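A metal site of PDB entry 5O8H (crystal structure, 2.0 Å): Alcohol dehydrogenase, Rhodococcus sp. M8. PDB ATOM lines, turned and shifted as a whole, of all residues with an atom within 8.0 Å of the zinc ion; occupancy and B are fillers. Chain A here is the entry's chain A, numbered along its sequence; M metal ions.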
ATOM      1  N   TRP A  90     -10.834  28.565  -0.710  1.00  0.00           N
ATOM      2  CA  TRP A  90      -9.477  28.162  -1.128  1.00  0.00           C
ATOM      3  C   TRP A  90      -8.559  27.900   0.045  1.00  0.00           C
ATOM      4  O   TRP A  90      -8.497  28.689   0.994  1.00  0.00           O
ATOM      5  CB  TRP A  90      -8.823  29.229  -2.030  1.00  0.00           C
ATOM      6  CG  TRP A  90      -9.566  29.468  -3.344  1.00  0.00           C
ATOM      7  CD1 TRP A  90     -10.592  28.743  -3.870  1.00  0.00           C
ATOM      8  CD2 TRP A  90      -9.286  30.510  -4.285  1.00  0.00           C
ATOM      9  NE1 TRP A  90     -10.981  29.271  -5.063  1.00  0.00           N
ATOM     10  CE2 TRP A  90     -10.194  30.357  -5.348  1.00  0.00           C
ATOM     11  CE3 TRP A  90      -8.370  31.566  -4.316  1.00  0.00           C
ATOM     12  CZ2 TRP A  90     -10.223  31.240  -6.452  1.00  0.00           C
ATOM     13  CZ3 TRP A  90      -8.390  32.446  -5.415  1.00  0.00           C
ATOM     14  CH2 TRP A  90      -9.305  32.271  -6.458  1.00  0.00           C
ATOM     15  N   GLY A  91      -7.847  26.775  -0.038  1.00  0.00           N
ATOM     16  CA  GLY A  91      -6.868  26.408   0.974  1.00  0.00           C
ATOM     17  C   GLY A  91      -5.491  26.268   0.369  1.00  0.00           C
ATOM     18  O   GLY A  91      -5.293  26.505  -0.832  1.00  0.00           O
ATOM     19  N   CYS A  92      -4.541  25.871   1.212  1.00  0.00           N
ATOM     20  CA  CYS A  92      -3.151  25.720   0.801  1.00  0.00           C
ATOM     21  C   CYS A  92      -2.922  24.569  -0.170  1.00  0.00           C
ATOM     22  O   CYS A  92      -1.965  24.591  -0.935  1.00  0.00           O
ATOM     23  CB  CYS A  92      -2.235  25.607   2.021  1.00  0.00           C
ATOM     24  SG  CYS A  92      -2.217  24.003   2.815  1.00  0.00           S
ATOM     25  N   GLY A  93      -3.781  23.559  -0.127  1.00  0.00           N
ATOM     26  CA  GLY A  93      -3.646  22.401  -1.027  1.00  0.00           C
ATOM     27  C   GLY A  93      -2.691  21.310  -0.567  1.00  0.00           C
ATOM     28  O   GLY A  93      -2.650  20.248  -1.196  1.00  0.00           O
ATOM     29  N   ALA A  94      -1.940  21.553   0.506  1.00  0.00           N
ATOM     30  CA  ALA A  94      -0.793  20.704   0.907  1.00  0.00           C
ATOM     31  C   ALA A  94      -0.921  20.037   2.291  1.00  0.00           C
ATOM     32  O   ALA A  94      -0.322  18.978   2.513  1.00  0.00           O
ATOM     33  CB  ALA A  94       0.488  21.544   0.875  1.00  0.00           C
ATOM     34  N   CYS A  95      -1.691  20.644   3.204  1.00  0.00           N
ATOM     35  CA  CYS A  95      -1.829  20.160   4.569  1.00  0.00           C
ATOM     36  C   CYS A  95      -2.728  18.908   4.622  1.00  0.00           C
ATOM     37  O   CYS A  95      -3.303  18.485   3.621  1.00  0.00           O
ATOM     38  CB  CYS A  95      -2.385  21.267   5.472  1.00  0.00           C
ATOM     39  SG  CYS A  95      -4.158  21.674   5.171  1.00  0.00           S
ATOM     40  N   HIS A  96      -2.841  18.319   5.805  1.00  0.00           N
ATOM     41  CA  HIS A  96      -3.583  17.075   5.964  1.00  0.00           C
ATOM     42  C   HIS A  96      -5.074  17.226   5.577  1.00  0.00           C
ATOM     43  O   HIS A  96      -5.640  16.379   4.885  1.00  0.00           O
ATOM     44  CB  HIS A  96      -3.401  16.554   7.383  1.00  0.00           C
ATOM     45  CG  HIS A  96      -4.025  15.213   7.637  1.00  0.00           C
ATOM     46  ND1 HIS A  96      -5.316  15.061   8.095  1.00  0.00           N
ATOM     47  CD2 HIS A  96      -3.518  13.955   7.535  1.00  0.00           C
ATOM     48  CE1 HIS A  96      -5.586  13.774   8.236  1.00  0.00           C
ATOM     49  NE2 HIS A  96      -4.505  13.083   7.908  1.00  0.00           N
ATOM     50  N   ALA A  97      -5.693  18.329   5.997  1.00  0.00           N
ATOM     51  CA  ALA A  97      -7.072  18.630   5.608  1.00  0.00           C
ATOM     52  C   ALA A  97      -7.211  18.831   4.098  1.00  0.00           C
ATOM     53  O   ALA A  97      -8.096  18.212   3.459  1.00  0.00           O
ATOM     54  CB  ALA A  97      -7.579  19.872   6.365  1.00  0.00           C
ATOM     55  N   CYS A  98      -6.342  19.660   3.513  1.00  0.00           N
ATOM     56  CA  CYS A  98      -6.380  19.909   2.065  1.00  0.00           C
ATOM     57  C   CYS A  98      -6.134  18.641   1.221  1.00  0.00           C
ATOM     58  O   CYS A  98      -6.755  18.469   0.156  1.00  0.00           O
ATOM     59  CB  CYS A  98      -5.410  21.036   1.623  1.00  0.00           C
ATOM     60  SG  CYS A  98      -5.919  22.710   2.144  1.00  0.00           S
ATOM     61  N   ALA A  99      -5.277  17.747   1.715  1.00  0.00           N
ATOM     62  CA  ALA A  99      -5.005  16.493   1.016  1.00  0.00           C
ATOM     63  C   ALA A  99      -6.261  15.619   0.888  1.00  0.00           C
ATOM     64  O   ALA A  99      -6.364  14.838  -0.050  1.00  0.00           O
ATOM     65  CB  ALA A  99      -3.886  15.724   1.692  1.00  0.00           C
ATOM     66  N   ARG A 102     -10.484  18.868   1.981  1.00  0.00           N
ATOM     67  CA  ARG A 102     -11.198  19.644   2.998  1.00  0.00           C
ATOM     68  C   ARG A 102     -10.562  20.990   3.171  1.00  0.00           C
ATOM     69  O   ARG A 102     -10.159  21.387   4.280  1.00  0.00           O
ATOM     70  CB  ARG A 102     -11.238  18.877   4.341  1.00  0.00           C
ATOM     71  CG  ARG A 102     -11.764  17.473   4.234  1.00  0.00           C
ATOM     72  CD  ARG A 102     -11.598  16.702   5.538  1.00  0.00           C
ATOM     73  NE  ARG A 102     -12.473  17.176   6.610  1.00  0.00           N
ATOM     74  CZ  ARG A 102     -13.773  16.903   6.712  1.00  0.00           C
ATOM     75  NH1 ARG A 102     -14.391  16.201   5.766  1.00  0.00           N
ATOM     76  NH2 ARG A 102     -14.469  17.379   7.752  1.00  0.00           N
ATOM     77  N   GLU A 103     -10.507  21.736   2.072  1.00  0.00           N
ATOM     78  CA  GLU A 103      -9.838  23.038   2.066  1.00  0.00           C
ATOM     79  C   GLU A 103     -10.602  24.075   2.890  1.00  0.00           C
ATOM     80  O   GLU A 103     -10.024  25.057   3.356  1.00  0.00           O
ATOM     81  CB  GLU A 103      -9.603  23.541   0.631  1.00  0.00           C
ATOM     82  CG  GLU A 103      -8.811  22.552  -0.211  1.00  0.00           C
ATOM     83  CD  GLU A 103      -8.066  23.170  -1.396  1.00  0.00           C
ATOM     84  OE1 GLU A 103      -8.122  24.421  -1.582  1.00  0.00           O
ATOM     85  OE2 GLU A 103      -7.426  22.391  -2.131  1.00  0.00           O
ATOM     86  N   ASN A 104     -11.893  23.826   3.091  1.00  0.00           N
ATOM     87  CA  ASN A 104     -12.683  24.611   4.039  1.00  0.00           C
ATOM     88  C   ASN A 104     -12.137  24.601   5.467  1.00  0.00           C
ATOM     89  O   ASN A 104     -12.375  25.538   6.211  1.00  0.00           O
ATOM     90  CB  ASN A 104     -14.165  24.162   4.020  1.00  0.00           C
ATOM     91  CG  ASN A 104     -14.373  22.671   4.304  1.00  0.00           C
ATOM     92  OD1 ASN A 104     -13.588  21.823   3.855  1.00  0.00           O
ATOM     93  ND2 ASN A 104     -15.445  22.353   5.012  1.00  0.00           N
ATOM     94  N   TYR A 105     -11.400  23.559   5.831  1.00  0.00           N
ATOM     95  CA  TYR A 105     -10.789  23.473   7.170  1.00  0.00           C
ATOM     96  C   TYR A 105      -9.263  23.565   7.134  1.00  0.00           C
ATOM     97  O   TYR A 105      -8.592  23.052   8.030  1.00  0.00           O
ATOM     98  CB  TYR A 105     -11.259  22.175   7.856  1.00  0.00           C
ATOM     99  CG  TYR A 105     -12.770  22.100   8.099  1.00  0.00           C
ATOM    100  CD1 TYR A 105     -13.440  23.164   8.723  1.00  0.00           C
ATOM    101  CD2 TYR A 105     -13.511  20.985   7.746  1.00  0.00           C
ATOM    102  CE1 TYR A 105     -14.809  23.119   8.947  1.00  0.00           C
ATOM    103  CE2 TYR A 105     -14.886  20.918   7.990  1.00  0.00           C
ATOM    104  CZ  TYR A 105     -15.523  21.998   8.586  1.00  0.00           C
ATOM    105  OH  TYR A 105     -16.878  21.963   8.795  1.00  0.00           O
ATOM    106  N   CYS A 106      -8.721  24.220   6.106  1.00  0.00           N
ATOM    107  CA  CYS A 106      -7.266  24.412   6.003  1.00  0.00           C
ATOM    108  C   CYS A 106      -6.805  25.369   7.111  1.00  0.00           C
ATOM    109  O   CYS A 106      -7.390  26.430   7.271  1.00  0.00           O
ATOM    110  CB  CYS A 106      -6.934  25.062   4.673  1.00  0.00           C
ATOM    111  SG  CYS A 106      -5.176  25.420   4.485  1.00  0.00           S
ATOM    112  N   THR A 107      -5.746  25.024   7.844  1.00  0.00           N
ATOM    113  CA  THR A 107      -5.187  25.947   8.872  1.00  0.00           C
ATOM    114  C   THR A 107      -4.028  26.825   8.380  1.00  0.00           C
ATOM    115  O   THR A 107      -3.664  27.786   9.067  1.00  0.00           O
ATOM    116  CB  THR A 107      -4.677  25.157  10.079  1.00  0.00           C
ATOM    117  OG1 THR A 107      -3.796  24.116   9.642  1.00  0.00           O
ATOM    118  CG2 THR A 107      -5.829  24.502  10.809  1.00  0.00           C
ATOM    119  N   ARG A 108      -3.504  26.540   7.189  1.00  0.00           N
ATOM    120  CA  ARG A 108      -2.334  27.263   6.669  1.00  0.00           C
ATOM    121  C   ARG A 108      -2.686  28.446   5.767  1.00  0.00           C
ATOM    122  O   ARG A 108      -1.805  29.276   5.505  1.00  0.00           O
ATOM    123  CB  ARG A 108      -1.423  26.280   5.935  1.00  0.00           C
ATOM    124  CG  ARG A 108      -0.952  25.154   6.815  1.00  0.00           C
ATOM    125  CD  ARG A 108       0.360  24.571   6.288  1.00  0.00           C
ATOM    126  NE  ARG A 108       1.283  25.600   5.806  1.00  0.00           N
ATOM    127  CZ  ARG A 108       2.269  26.129   6.530  1.00  0.00           C
ATOM    128  NH1 ARG A 108       3.051  27.045   5.997  1.00  0.00           N
ATOM    129  NH2 ARG A 108       2.478  25.722   7.766  1.00  0.00           N
ATOM    130  N   ALA A 109      -3.926  28.528   5.286  1.00  0.00           N
ATOM    131  CA  ALA A 109      -4.302  29.538   4.265  1.00  0.00           C
ATOM    132  C   ALA A 109      -4.012  30.998   4.673  1.00  0.00           C
ATOM    133  O   ALA A 109      -3.429  31.764   3.880  1.00  0.00           O
ATOM    134  CB  ALA A 109      -5.774  29.386   3.854  1.00  0.00           C
ATOM    135  N   LEU A 112      -0.330  31.935   4.631  1.00  0.00           N
ATOM    136  CA  LEU A 112       0.192  31.969   3.264  1.00  0.00           C
ATOM    137  C   LEU A 112      -0.444  33.091   2.412  1.00  0.00           C
ATOM    138  O   LEU A 112      -0.100  33.216   1.229  1.00  0.00           O
ATOM    139  CB  LEU A 112      -0.008  30.612   2.583  1.00  0.00           C
ATOM    140  CG  LEU A 112       0.805  29.452   3.179  1.00  0.00           C
ATOM    141  CD1 LEU A 112       0.349  28.138   2.565  1.00  0.00           C
ATOM    142  CD2 LEU A 112       2.309  29.647   2.978  1.00  0.00           C
ATOM    143  N   ILE A 114      -3.607  33.274   1.424  1.00  0.00           N
ATOM    144  CA  ILE A 114      -4.620  32.726   0.532  1.00  0.00           C
ATOM    145  C   ILE A 114      -5.961  33.213   1.053  1.00  0.00           C
ATOM    146  O   ILE A 114      -6.296  32.987   2.206  1.00  0.00           O
ATOM    147  CB  ILE A 114      -4.544  31.185   0.461  1.00  0.00           C
ATOM    148  CG1 ILE A 114      -3.180  30.780  -0.152  1.00  0.00           C
ATOM    149  CG2 ILE A 114      -5.691  30.611  -0.384  1.00  0.00           C
ATOM    150  CD1 ILE A 114      -2.820  29.316  -0.027  1.00  0.00           C
ATOM    151  N   ARG A 135      -7.500  22.991  -9.548  1.00  0.00           N
ATOM    152  CA  ARG A 135      -8.200  22.181  -8.546  1.00  0.00           C
ATOM    153  C   ARG A 135      -9.397  22.909  -7.925  1.00  0.00           C
ATOM    154  O   ARG A 135     -10.195  22.286  -7.239  1.00  0.00           O
ATOM    155  CB  ARG A 135      -7.234  21.672  -7.471  1.00  0.00           C
ATOM    156  CG  ARG A 135      -6.917  22.643  -6.357  1.00  0.00           C
ATOM    157  CD  ARG A 135      -5.909  22.076  -5.385  1.00  0.00           C
ATOM    158  NE  ARG A 135      -5.791  23.000  -4.251  1.00  0.00           N
ATOM    159  CZ  ARG A 135      -5.015  24.069  -4.203  1.00  0.00           C
ATOM    160  NH1 ARG A 135      -4.219  24.388  -5.218  1.00  0.00           N
ATOM    161  NH2 ARG A 135      -5.024  24.834  -3.110  1.00  0.00           N
HETATM  162 ZN    ZN M   1      -4.297  23.426   3.673  1.00  0.00          ZN
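The side-chain sulfur (SG) of Cys 95 lies close to the backbone NH (N) of Ala 97, 3.8 Å away.
SG of Cys 92 sits close to N of Ala 94 (3.4 Å).
SG of Cys 106 lies close to N of Arg 108.
The side-chain sulfur (SG) of Cys 106 lies close to the backbone NH (N) of Ala 109 (3.4 Å).
The side-chain sulfur of Cys 98 sits close to the backbone NH of Gly 93 (3.2 Å).
Gly 93 touches the zinc ion (N to ZN, 3.8 Å).
The zinc ion is bound by SG of Cys 95 (2.3 Å), SG of Cys 92 (2.3 Å), SG of Cys 106 (2.3 Å) and SG of Cys 98 (2.3 Å).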
